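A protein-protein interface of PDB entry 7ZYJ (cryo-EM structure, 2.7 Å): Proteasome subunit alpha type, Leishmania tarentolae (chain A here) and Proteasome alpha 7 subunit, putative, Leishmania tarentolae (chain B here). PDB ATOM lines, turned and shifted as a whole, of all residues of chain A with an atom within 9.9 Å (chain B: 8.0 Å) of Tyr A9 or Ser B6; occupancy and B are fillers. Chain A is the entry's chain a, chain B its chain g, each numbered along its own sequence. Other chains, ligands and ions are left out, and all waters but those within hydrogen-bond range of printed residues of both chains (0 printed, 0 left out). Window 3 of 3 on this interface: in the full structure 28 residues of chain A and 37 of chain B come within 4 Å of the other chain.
The side-chain hydroxyl of Tyr A9 sits at hydrogen-bond distance from the side-chain hydroxyl of Ser B6, at 2.8 Å. N of Phe B15 lies within hydrogen-bond range of OE1 of Gln A21.
The backbone carbonyl oxygen (O) of Lys A8 sits at hydrogen-bond distance from the side-chain amide nitrogen (NE2) of Gln A21, 3.0 Å away. The backbone carbonyl oxygen (O) of Arg A129 lies within hydrogen-bond range of the guanidinium group (NE) of Arg A122 (2.5 Å). OG of Ser B6 lies within hydrogen-bond range of ND1 of His B8, 2.9 Å away. The backbone carbonyl oxygen (O) of Ser B6 is in hydrogen-bond range of the side-chain amide nitrogen (NE2) of Gln B10. OG of Ser B11 is in hydrogen-bond range of OD1 of Asp B13 (2.9 Å).
Among the printed residues, pairs that only touch across the chains: Pro A130 with Phe B15 (3.1 Å), Arg A129 with Thr B12 (3.1 Å), Arg A129 with Phe B15 (3.2 Å), Tyr A24 with Ser B16 (3.2 Å), Tyr A9 with Val B14 (3.3 Å), Gly A127 with Asp B13 (3.3 Å), Gln A21 with Val B14 (3.4 Å), Tyr A24 with Phe B15 (3.5 Å), Arg A129 with Asp B13 (3.5 Å), Tyr A9 with Gly B7 (3.6 Å), Gln A21 with Asp B13 (3.6 Å), Tyr A24 with Ala B17 (3.7 Å), Tyr A9 with His B8 (3.8 Å) and Ala A126 with Asp B13 (3.8 Å).
Phe A6 touches none of the printed residues of chain B. Of the printed residues of chain B, Tyr A9 touches Ser B6 (2.8 Å), Gly B7 (3.6 Å), His B8 (3.8 Å) and Val B14 (3.3 Å). Val A22 touches none of the printed residues of chain B. Printed residues of chain B within 4 Å of Tyr A24: Phe B15, Ser B16 and Ala B17. Of chain A, only Tyr A9 (2.8 Å) comes within 4 Å of Ser B6. Of chain A, only Tyr A9 (3.6 Å) comes within 4 Å of Gly B7. Of the printed residues of chain A, Ser B16 touches Tyr A24. Printed residues of chain A within 4 Å of Ala B17: Tyr A24. The nearest residue of chain B that does not touch Tyr A9 is Asp B13 (4.4 Å).
Of the 13 printed residues of chain B, 9 touch a printed residue of chain A. Hydrophobic or aromatic side chains of chain B within 4 Å of the printed part of chain A: His B8, Val B14 and Phe B15. Along chain A the printed residues that touch a printed residue of chain B span positions 9 to 130.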
ATOM      1  N   ALA A   4      25.533 -13.417   6.661  1.00  0.00           N
ATOM      2  CA  ALA A   4      25.122 -13.959   5.371  1.00  0.00           C
ATOM      3  C   ALA A   4      24.313 -15.238   5.551  1.00  0.00           C
ATOM      4  O   ALA A   4      23.903 -15.868   4.576  1.00  0.00           O
ATOM      5  CB  ALA A   4      26.336 -14.217   4.491  1.00  0.00           C
ATOM      6  N   GLY A   5      24.089 -15.618   6.805  1.00  0.00           N
ATOM      7  CA  GLY A   5      23.360 -16.834   7.104  1.00  0.00           C
ATOM      8  C   GLY A   5      21.882 -16.618   7.349  1.00  0.00           C
ATOM      9  O   GLY A   5      21.051 -17.414   6.902  1.00  0.00           O
ATOM     10  N   PHE A   6      21.537 -15.544   8.060  1.00  0.00           N
ATOM     11  CA  PHE A   6      20.142 -15.322   8.441  1.00  0.00           C
ATOM     12  C   PHE A   6      19.340 -14.696   7.302  1.00  0.00           C
ATOM     13  O   PHE A   6      18.358 -15.276   6.835  1.00  0.00           O
ATOM     14  CB  PHE A   6      20.075 -14.458   9.708  1.00  0.00           C
ATOM     15  CG  PHE A   6      21.098 -13.347   9.755  1.00  0.00           C
ATOM     16  CD1 PHE A   6      22.379 -13.582  10.231  1.00  0.00           C
ATOM     17  CD2 PHE A   6      20.770 -12.064   9.343  1.00  0.00           C
ATOM     18  CE1 PHE A   6      23.316 -12.566  10.277  1.00  0.00           C
ATOM     19  CE2 PHE A   6      21.704 -11.045   9.386  1.00  0.00           C
ATOM     20  CZ  PHE A   6      22.978 -11.297   9.854  1.00  0.00           C
ATOM     21  N   ASP A   7      19.711 -13.475   6.906  1.00  0.00           N
ATOM     22  CA  ASP A   7      19.230 -12.707   5.753  1.00  0.00           C
ATOM     23  C   ASP A   7      17.708 -12.588   5.715  1.00  0.00           C
ATOM     24  O   ASP A   7      17.147 -12.118   4.720  1.00  0.00           O
ATOM     25  CB  ASP A   7      19.794 -13.261   4.423  1.00  0.00           C
ATOM     26  CG  ASP A   7      19.066 -14.500   3.876  1.00  0.00           C
ATOM     27  OD1 ASP A   7      18.047 -14.969   4.414  1.00  0.00           O
ATOM     28  OD2 ASP A   7      19.547 -15.023   2.849  1.00  0.00           O
ATOM     29  N   LYS A   8      17.030 -13.004   6.788  1.00  0.00           N
ATOM     30  CA  LYS A   8      15.573 -12.977   6.809  1.00  0.00           C
ATOM     31  C   LYS A   8      15.001 -12.552   8.157  1.00  0.00           C
ATOM     32  O   LYS A   8      13.775 -12.551   8.317  1.00  0.00           O
ATOM     33  CB  LYS A   8      15.007 -14.348   6.420  1.00  0.00           C
ATOM     34  CG  LYS A   8      15.209 -15.432   7.461  1.00  0.00           C
ATOM     35  CD  LYS A   8      14.659 -16.761   6.972  1.00  0.00           C
ATOM     36  CE  LYS A   8      15.116 -17.057   5.552  1.00  0.00           C
ATOM     37  NZ  LYS A   8      14.536 -18.326   5.035  1.00  0.00           N
ATOM     38  N   TYR A   9      15.839 -12.194   9.129  1.00  0.00           N
ATOM     39  CA  TYR A   9      15.364 -11.679  10.404  1.00  0.00           C
ATOM     40  C   TYR A   9      15.388 -10.159  10.471  1.00  0.00           C
ATOM     41  O   TYR A   9      14.729  -9.583  11.342  1.00  0.00           O
ATOM     42  CB  TYR A   9      16.198 -12.251  11.558  1.00  0.00           C
ATOM     43  CG  TYR A   9      16.240 -13.760  11.600  1.00  0.00           C
ATOM     44  CD1 TYR A   9      15.133 -14.516  11.238  1.00  0.00           C
ATOM     45  CD2 TYR A   9      17.385 -14.430  12.007  1.00  0.00           C
ATOM     46  CE1 TYR A   9      15.168 -15.896  11.276  1.00  0.00           C
ATOM     47  CE2 TYR A   9      17.429 -15.810  12.048  1.00  0.00           C
ATOM     48  CZ  TYR A   9      16.317 -16.538  11.682  1.00  0.00           C
ATOM     49  OH  TYR A   9      16.355 -17.912  11.722  1.00  0.00           O
ATOM     50  N   ILE A  10      16.126  -9.502   9.578  1.00  0.00           N
ATOM     51  CA  ILE A  10      16.187  -8.051   9.507  1.00  0.00           C
ATOM     52  C   ILE A  10      15.970  -7.629   8.059  1.00  0.00           C
ATOM     53  O   ILE A  10      16.052  -8.435   7.132  1.00  0.00           O
ATOM     54  CB  ILE A  10      17.517  -7.487  10.046  1.00  0.00           C
ATOM     55  CG1 ILE A  10      18.694  -7.994   9.212  1.00  0.00           C
ATOM     56  CG2 ILE A  10      17.688  -7.832  11.514  1.00  0.00           C
ATOM     57  CD1 ILE A  10      20.002  -7.309   9.531  1.00  0.00           C
ATOM     58  N   THR A  11      15.686  -6.341   7.878  1.00  0.00           N
ATOM     59  CA  THR A  11      15.352  -5.795   6.564  1.00  0.00           C
ATOM     60  C   THR A  11      16.626  -5.686   5.731  1.00  0.00           C
ATOM     61  O   THR A  11      17.213  -4.616   5.555  1.00  0.00           O
ATOM     62  CB  THR A  11      14.657  -4.446   6.703  1.00  0.00           C
ATOM     63  OG1 THR A  11      15.341  -3.654   7.682  1.00  0.00           O
ATOM     64  CG2 THR A  11      13.210  -4.636   7.132  1.00  0.00           C
ATOM     65  N   VAL A  12      17.060  -6.832   5.212  1.00  0.00           N
ATOM     66  CA  VAL A  12      18.161  -6.905   4.263  1.00  0.00           C
ATOM     67  C   VAL A  12      17.708  -7.750   3.082  1.00  0.00           C
ATOM     68  O   VAL A  12      16.823  -8.601   3.206  1.00  0.00           O
ATOM     69  CB  VAL A  12      19.444  -7.491   4.894  1.00  0.00           C
ATOM     70  CG1 VAL A  12      20.028  -6.521   5.909  1.00  0.00           C
ATOM     71  CG2 VAL A  12      19.155  -8.836   5.538  1.00  0.00           C
ATOM     72  N   PHE A  13      18.317  -7.503   1.927  1.00  0.00           N
ATOM     73  CA  PHE A  13      17.930  -8.220   0.720  1.00  0.00           C
ATOM     74  C   PHE A  13      18.367  -9.677   0.781  1.00  0.00           C
ATOM     75  O   PHE A  13      19.465 -10.000   1.245  1.00  0.00           O
ATOM     76  CB  PHE A  13      18.530  -7.556  -0.516  1.00  0.00           C
ATOM     77  CG  PHE A  13      17.882  -6.257  -0.880  1.00  0.00           C
ATOM     78  CD1 PHE A  13      16.712  -6.237  -1.618  1.00  0.00           C
ATOM     79  CD2 PHE A  13      18.445  -5.056  -0.495  1.00  0.00           C
ATOM     80  CE1 PHE A  13      16.113  -5.042  -1.958  1.00  0.00           C
ATOM     81  CE2 PHE A  13      17.851  -3.861  -0.832  1.00  0.00           C
ATOM     82  CZ  PHE A  13      16.683  -3.853  -1.565  1.00  0.00           C
ATOM     83  N   SER A  14      17.493 -10.555   0.310  1.00  0.00           N
ATOM     84  CA  SER A  14      17.834 -11.946   0.069  1.00  0.00           C
ATOM     85  C   SER A  14      18.629 -12.051  -1.225  1.00  0.00           C
ATOM     86  O   SER A  14      18.678 -11.106  -2.015  1.00  0.00           O
ATOM     87  CB  SER A  14      16.559 -12.784   0.013  1.00  0.00           C
ATOM     88  OG  SER A  14      15.779 -12.449  -1.122  1.00  0.00           O
ATOM     89  N   SER A  18      14.655 -10.038  -2.524  1.00  0.00           N
ATOM     90  CA  SER A  18      13.377  -9.916  -1.844  1.00  0.00           C
ATOM     91  C   SER A  18      13.610  -9.657  -0.363  1.00  0.00           C
ATOM     92  O   SER A  18      14.665  -9.978   0.188  1.00  0.00           O
ATOM     93  CB  SER A  18      12.517 -11.173  -2.032  1.00  0.00           C
ATOM     94  OG  SER A  18      13.091 -12.284  -1.368  1.00  0.00           O
ATOM     95  N   LEU A  19      12.606  -9.066   0.277  1.00  0.00           N
ATOM     96  CA  LEU A  19      12.638  -8.767   1.704  1.00  0.00           C
ATOM     97  C   LEU A  19      11.741  -9.772   2.415  1.00  0.00           C
ATOM     98  O   LEU A  19      10.514  -9.721   2.284  1.00  0.00           O
ATOM     99  CB  LEU A  19      12.186  -7.334   1.969  1.00  0.00           C
ATOM    100  CG  LEU A  19      12.994  -6.230   1.286  1.00  0.00           C
ATOM    101  CD1 LEU A  19      12.240  -4.912   1.334  1.00  0.00           C
ATOM    102  CD2 LEU A  19      14.362  -6.093   1.931  1.00  0.00           C
ATOM    103  N   TYR A  20      12.359 -10.689   3.164  1.00  0.00           N
ATOM    104  CA  TYR A  20      11.597 -11.750   3.812  1.00  0.00           C
ATOM    105  C   TYR A  20      10.730 -11.209   4.941  1.00  0.00           C
ATOM    106  O   TYR A  20       9.601 -11.673   5.139  1.00  0.00           O
ATOM    107  CB  TYR A  20      12.545 -12.828   4.334  1.00  0.00           C
ATOM    108  CG  TYR A  20      12.875 -13.891   3.314  1.00  0.00           C
ATOM    109  CD1 TYR A  20      11.892 -14.737   2.822  1.00  0.00           C
ATOM    110  CD2 TYR A  20      14.171 -14.047   2.841  1.00  0.00           C
ATOM    111  CE1 TYR A  20      12.191 -15.710   1.889  1.00  0.00           C
ATOM    112  CE2 TYR A  20      14.479 -15.016   1.908  1.00  0.00           C
ATOM    113  CZ  TYR A  20      13.484 -15.845   1.435  1.00  0.00           C
ATOM    114  OH  TYR A  20      13.786 -16.813   0.505  1.00  0.00           O
ATOM    115  N   GLN A  21      11.240 -10.237   5.701  1.00  0.00           N
ATOM    116  CA  GLN A  21      10.472  -9.681   6.808  1.00  0.00           C
ATOM    117  C   GLN A  21       9.242  -8.921   6.336  1.00  0.00           C
ATOM    118  O   GLN A  21       8.297  -8.753   7.113  1.00  0.00           O
ATOM    119  CB  GLN A  21      11.356  -8.767   7.656  1.00  0.00           C
ATOM    120  CG  GLN A  21      12.144  -9.501   8.724  1.00  0.00           C
ATOM    121  CD  GLN A  21      11.247 -10.210   9.716  1.00  0.00           C
ATOM    122  OE1 GLN A  21      10.476  -9.577  10.436  1.00  0.00           O
ATOM    123  NE2 GLN A  21      11.341 -11.533   9.756  1.00  0.00           N
ATOM    124  N   VAL A  22       9.229  -8.459   5.088  1.00  0.00           N
ATOM    125  CA  VAL A  22       8.045  -7.804   4.549  1.00  0.00           C
ATOM    126  C   VAL A  22       7.063  -8.816   3.966  1.00  0.00           C
ATOM    127  O   VAL A  22       5.847  -8.616   4.052  1.00  0.00           O
ATOM    128  CB  VAL A  22       8.445  -6.754   3.502  1.00  0.00           C
ATOM    129  CG1 VAL A  22       7.259  -5.884   3.159  1.00  0.00           C
ATOM    130  CG2 VAL A  22       9.587  -5.902   4.024  1.00  0.00           C
ATOM    131  N   TYR A  24       6.709 -11.783   5.217  1.00  0.00           N
ATOM    132  CA  TYR A  24       6.119 -12.391   6.403  1.00  0.00           C
ATOM    133  C   TYR A  24       5.043 -11.505   7.014  1.00  0.00           C
ATOM    134  O   TYR A  24       4.066 -12.018   7.571  1.00  0.00           O
ATOM    135  CB  TYR A  24       7.203 -12.690   7.439  1.00  0.00           C
ATOM    136  CG  TYR A  24       8.180 -13.768   7.023  1.00  0.00           C
ATOM    137  CD1 TYR A  24       7.934 -14.570   5.918  1.00  0.00           C
ATOM    138  CD2 TYR A  24       9.350 -13.981   7.738  1.00  0.00           C
ATOM    139  CE1 TYR A  24       8.824 -15.553   5.538  1.00  0.00           C
ATOM    140  CE2 TYR A  24      10.246 -14.961   7.366  1.00  0.00           C
ATOM    141  CZ  TYR A  24       9.978 -15.744   6.265  1.00  0.00           C
ATOM    142  OH  TYR A  24      10.868 -16.724   5.891  1.00  0.00           O
ATOM    143  N   ARG A 122       9.984   1.558   7.771  1.00  0.00           N
ATOM    144  CA  ARG A 122      10.182   0.368   8.589  1.00  0.00           C
ATOM    145  C   ARG A 122      10.712  -0.817   7.793  1.00  0.00           C
ATOM    146  O   ARG A 122      11.120  -1.811   8.400  1.00  0.00           O
ATOM    147  CB  ARG A 122       8.871  -0.014   9.280  1.00  0.00           C
ATOM    148  CG  ARG A 122       8.233   1.126  10.055  1.00  0.00           C
ATOM    149  CD  ARG A 122       7.030   0.657  10.854  1.00  0.00           C
ATOM    150  NE  ARG A 122       7.413  -0.212  11.959  1.00  0.00           N
ATOM    151  CZ  ARG A 122       7.853   0.220  13.134  1.00  0.00           C
ATOM    152  NH1 ARG A 122       7.977   1.510  13.392  1.00  0.00           N
ATOM    153  NH2 ARG A 122       8.177  -0.667  14.071  1.00  0.00           N
ATOM    154  N   GLN A 125      14.901   0.591   7.667  1.00  0.00           N
ATOM    155  CA  GLN A 125      15.571   0.620   8.957  1.00  0.00           C
ATOM    156  C   GLN A 125      15.551  -0.773   9.575  1.00  0.00           C
ATOM    157  O   GLN A 125      14.556  -1.497   9.487  1.00  0.00           O
ATOM    158  CB  GLN A 125      14.899   1.629   9.888  1.00  0.00           C
ATOM    159  CG  GLN A 125      15.562   1.798  11.247  1.00  0.00           C
ATOM    160  CD  GLN A 125      16.981   2.321  11.152  1.00  0.00           C
ATOM    161  OE1 GLN A 125      17.942   1.573  11.330  1.00  0.00           O
ATOM    162  NE2 GLN A 125      17.119   3.610  10.870  1.00  0.00           N
ATOM    163  N   ALA A 126      16.665  -1.141  10.209  1.00  0.00           N
ATOM    164  CA  ALA A 126      16.861  -2.523  10.633  1.00  0.00           C
ATOM    165  C   ALA A 126      16.002  -2.887  11.839  1.00  0.00           C
ATOM    166  O   ALA A 126      15.384  -3.956  11.870  1.00  0.00           O
ATOM    167  CB  ALA A 126      18.339  -2.769  10.938  1.00  0.00           C
ATOM    168  N   GLY A 127      15.952  -2.013  12.847  1.00  0.00           N
ATOM    169  CA  GLY A 127      15.376  -2.407  14.121  1.00  0.00           C
ATOM    170  C   GLY A 127      13.860  -2.368  14.171  1.00  0.00           C
ATOM    171  O   GLY A 127      13.259  -2.878  15.119  1.00  0.00           O
ATOM    172  N   LEU A 128      13.224  -1.774  13.166  1.00  0.00           N
ATOM    173  CA  LEU A 128      11.780  -1.602  13.198  1.00  0.00           C
ATOM    174  C   LEU A 128      11.067  -2.762  12.512  1.00  0.00           C
ATOM    175  O   LEU A 128      11.495  -3.253  11.464  1.00  0.00           O
ATOM    176  CB  LEU A 128      11.379  -0.284  12.539  1.00  0.00           C
ATOM    177  CG  LEU A 128      12.262   0.919  12.868  1.00  0.00           C
ATOM    178  CD1 LEU A 128      11.951   2.078  11.937  1.00  0.00           C
ATOM    179  CD2 LEU A 128      12.080   1.325  14.320  1.00  0.00           C
ATOM    180  N   ARG A 129       9.959  -3.196  13.122  1.00  0.00           N
ATOM    181  CA  ARG A 129       9.130  -4.267  12.585  1.00  0.00           C
ATOM    182  C   ARG A 129       7.999  -3.685  11.756  1.00  0.00           C
ATOM    183  O   ARG A 129       7.329  -2.747  12.209  1.00  0.00           O
ATOM    184  CB  ARG A 129       8.552  -5.118  13.710  1.00  0.00           C
ATOM    185  CG  ARG A 129       7.891  -6.399  13.235  1.00  0.00           C
ATOM    186  CD  ARG A 129       7.140  -7.082  14.360  1.00  0.00           C
ATOM    187  NE  ARG A 129       5.706  -6.838  14.283  1.00  0.00           N
ATOM    188  CZ  ARG A 129       4.958  -6.434  15.301  1.00  0.00           C
ATOM    189  NH1 ARG A 129       5.479  -6.214  16.496  1.00  0.00           N
ATOM    190  NH2 ARG A 129       3.656  -6.247  15.114  1.00  0.00           N
ATOM    191  N   PRO A 130       7.758  -4.197  10.551  1.00  0.00           N
ATOM    192  CA  PRO A 130       6.626  -3.706   9.760  1.00  0.00           C
ATOM    193  C   PRO A 130       5.301  -4.034  10.427  1.00  0.00           C
ATOM    194  O   PRO A 130       5.174  -5.008  11.171  1.00  0.00           O
ATOM    195  CB  PRO A 130       6.773  -4.449   8.425  1.00  0.00           C
ATOM    196  CG  PRO A 130       8.186  -4.938   8.402  1.00  0.00           C
ATOM    197  CD  PRO A 130       8.544  -5.205   9.825  1.00  0.00           C
ATOM    198  N   SER B   6      15.262 -21.382  16.263  1.00  0.00           N
ATOM    199  CA  SER B   6      16.327 -20.615  15.631  1.00  0.00           C
ATOM    200  C   SER B   6      16.329 -19.171  16.121  1.00  0.00           C
ATOM    201  O   SER B   6      15.986 -18.895  17.270  1.00  0.00           O
ATOM    202  CB  SER B   6      16.184 -20.651  14.108  1.00  0.00           C
ATOM    203  OG  SER B   6      15.253 -19.680  13.663  1.00  0.00           O
ATOM    204  N   GLY B   7      16.719 -18.254  15.241  1.00  0.00           N
ATOM    205  CA  GLY B   7      16.758 -16.840  15.544  1.00  0.00           C
ATOM    206  C   GLY B   7      15.492 -16.077  15.226  1.00  0.00           C
ATOM    207  O   GLY B   7      15.507 -14.841  15.273  1.00  0.00           O
ATOM    208  N   HIS B   8      14.399 -16.764  14.906  1.00  0.00           N
ATOM    209  CA  HIS B   8      13.143 -16.120  14.549  1.00  0.00           C
ATOM    210  C   HIS B   8      12.265 -15.814  15.755  1.00  0.00           C
ATOM    211  O   HIS B   8      11.151 -15.311  15.577  1.00  0.00           O
ATOM    212  CB  HIS B   8      12.369 -16.995  13.559  1.00  0.00           C
ATOM    213  CG  HIS B   8      11.813 -18.245  14.166  1.00  0.00           C
ATOM    214  ND1 HIS B   8      12.611 -19.217  14.730  1.00  0.00           N
ATOM    215  CD2 HIS B   8      10.539 -18.683  14.298  1.00  0.00           C
ATOM    216  CE1 HIS B   8      11.852 -20.199  15.184  1.00  0.00           C
ATOM    217  NE2 HIS B   8      10.590 -19.899  14.933  1.00  0.00           N
ATOM    218  N   ASP B   9      12.734 -16.104  16.971  1.00  0.00           N
ATOM    219  CA  ASP B   9      11.932 -15.895  18.170  1.00  0.00           C
ATOM    220  C   ASP B   9      12.737 -15.228  19.278  1.00  0.00           C
ATOM    221  O   ASP B   9      12.368 -15.312  20.454  1.00  0.00           O
ATOM    222  CB  ASP B   9      11.348 -17.217  18.671  1.00  0.00           C
ATOM    223  CG  ASP B   9      12.416 -18.222  19.053  1.00  0.00           C
ATOM    224  OD1 ASP B   9      13.587 -18.029  18.666  1.00  0.00           O
ATOM    225  OD2 ASP B   9      12.085 -19.210  19.741  1.00  0.00           O
ATOM    226  N   GLN B  10      13.835 -14.560  18.926  1.00  0.00           N
ATOM    227  CA  GLN B  10      14.689 -13.919  19.916  1.00  0.00           C
ATOM    228  C   GLN B  10      14.330 -12.463  20.177  1.00  0.00           C
ATOM    229  O   GLN B  10      14.693 -11.934  21.233  1.00  0.00           O
ATOM    230  CB  GLN B  10      16.156 -14.005  19.483  1.00  0.00           C
ATOM    231  CG  GLN B  10      16.622 -15.415  19.169  1.00  0.00           C
ATOM    232  CD  GLN B  10      16.875 -16.236  20.416  1.00  0.00           C
ATOM    233  OE1 GLN B  10      17.388 -15.728  21.414  1.00  0.00           O
ATOM    234  NE2 GLN B  10      16.515 -17.513  20.368  1.00  0.00           N
ATOM    235  N   SER B  11      13.628 -11.806  19.255  1.00  0.00           N
ATOM    236  CA  SER B  11      13.261 -10.409  19.419  1.00  0.00           C
ATOM    237  C   SER B  11      11.889 -10.171  18.809  1.00  0.00           C
ATOM    238  O   SER B  11      11.422 -10.930  17.958  1.00  0.00           O
ATOM    239  CB  SER B  11      14.297  -9.473  18.784  1.00  0.00           C
ATOM    240  OG  SER B  11      14.700  -9.948  17.512  1.00  0.00           O
ATOM    241  N   THR B  12      11.243  -9.094  19.260  1.00  0.00           N
ATOM    242  CA  THR B  12       9.889  -8.780  18.823  1.00  0.00           C
ATOM    243  C   THR B  12       9.834  -8.181  17.427  1.00  0.00           C
ATOM    244  O   THR B  12       8.779  -8.239  16.788  1.00  0.00           O
ATOM    245  CB  THR B  12       9.230  -7.809  19.802  1.00  0.00           C
ATOM    246  OG1 THR B  12       9.942  -6.566  19.794  1.00  0.00           O
ATOM    247  CG2 THR B  12       9.268  -8.379  21.191  1.00  0.00           C
ATOM    248  N   ASP B  13      10.931  -7.610  16.941  1.00  0.00           N
ATOM    249  CA  ASP B  13      10.946  -6.955  15.641  1.00  0.00           C
ATOM    250  C   ASP B  13      11.022  -7.936  14.480  1.00  0.00           C
ATOM    251  O   ASP B  13      11.236  -7.507  13.341  1.00  0.00           O
ATOM    252  CB  ASP B  13      12.116  -5.970  15.564  1.00  0.00           C
ATOM    253  CG  ASP B  13      13.455  -6.665  15.441  1.00  0.00           C
ATOM    254  OD1 ASP B  13      13.822  -7.416  16.366  1.00  0.00           O
ATOM    255  OD2 ASP B  13      14.144  -6.458  14.420  1.00  0.00           O
ATOM    256  N   VAL B  14      10.847  -9.230  14.733  1.00  0.00           N
ATOM    257  CA  VAL B  14      11.004 -10.262  13.717  1.00  0.00           C
ATOM    258  C   VAL B  14       9.684 -11.004  13.572  1.00  0.00           C
ATOM    259  O   VAL B  14       9.133 -11.495  14.563  1.00  0.00           O
ATOM    260  CB  VAL B  14      12.136 -11.243  14.067  1.00  0.00           C
ATOM    261  CG1 VAL B  14      12.234 -12.340  13.021  1.00  0.00           C
ATOM    262  CG2 VAL B  14      13.455 -10.504  14.202  1.00  0.00           C
ATOM    263  N   PHE B  15       9.179 -11.082  12.345  1.00  0.00           N
ATOM    264  CA  PHE B  15       8.044 -11.938  12.042  1.00  0.00           C
ATOM    265  C   PHE B  15       8.513 -13.354  11.741  1.00  0.00           C
ATOM    266  O   PHE B  15       9.602 -13.571  11.203  1.00  0.00           O
ATOM    267  CB  PHE B  15       7.254 -11.401  10.848  1.00  0.00           C
ATOM    268  CG  PHE B  15       6.235 -10.359  11.205  1.00  0.00           C
ATOM    269  CD1 PHE B  15       5.118 -10.693  11.949  1.00  0.00           C
ATOM    270  CD2 PHE B  15       6.384  -9.052  10.779  1.00  0.00           C
ATOM    271  CE1 PHE B  15       4.175  -9.742  12.273  1.00  0.00           C
ATOM    272  CE2 PHE B  15       5.443  -8.096  11.100  1.00  0.00           C
ATOM    273  CZ  PHE B  15       4.336  -8.441  11.847  1.00  0.00           C
ATOM    274  N   SER B  16       7.678 -14.324  12.095  1.00  0.00           N
ATOM    275  CA  SER B  16       7.951 -15.704  11.734  1.00  0.00           C
ATOM    276  C   SER B  16       7.508 -15.965  10.298  1.00  0.00           C
ATOM    277  O   SER B  16       6.874 -15.128   9.651  1.00  0.00           O
ATOM    278  CB  SER B  16       7.249 -16.659  12.696  1.00  0.00           C
ATOM    279  OG  SER B  16       5.846 -16.620  12.518  1.00  0.00           O
ATOM    280  N   ALA B  17       7.856 -17.151   9.793  1.00  0.00           N
ATOM    281  CA  ALA B  17       7.485 -17.518   8.432  1.00  0.00           C
ATOM    282  C   ALA B  17       5.977 -17.559   8.232  1.00  0.00           C
ATOM    283  O   ALA B  17       5.509 -17.395   7.100  1.00  0.00           O
ATOM    284  CB  ALA B  17       8.094 -18.872   8.067  1.00  0.00           C
ATOM    285  N   TYR B  26       5.255 -15.749  23.874  1.00  0.00           N
ATOM    286  CA  TYR B  26       5.917 -16.196  25.097  1.00  0.00           C
ATOM    287  C   TYR B  26       5.507 -15.339  26.288  1.00  0.00           C
ATOM    288  O   TYR B  26       5.315 -15.854  27.398  1.00  0.00           O
ATOM    289  CB  TYR B  26       7.434 -16.175  24.910  1.00  0.00           C
ATOM    290  CG  TYR B  26       7.945 -17.082  23.811  1.00  0.00           C
ATOM    291  CD1 TYR B  26       7.146 -18.086  23.279  1.00  0.00           C
ATOM    292  CD2 TYR B  26       9.229 -16.931  23.305  1.00  0.00           C
ATOM    293  CE1 TYR B  26       7.612 -18.911  22.275  1.00  0.00           C
ATOM    294  CE2 TYR B  26       9.702 -17.754  22.303  1.00  0.00           C
ATOM    295  CZ  TYR B  26       8.890 -18.742  21.792  1.00  0.00           C
ATOM    296  OH  TYR B  26       9.356 -19.564  20.793  1.00  0.00           O
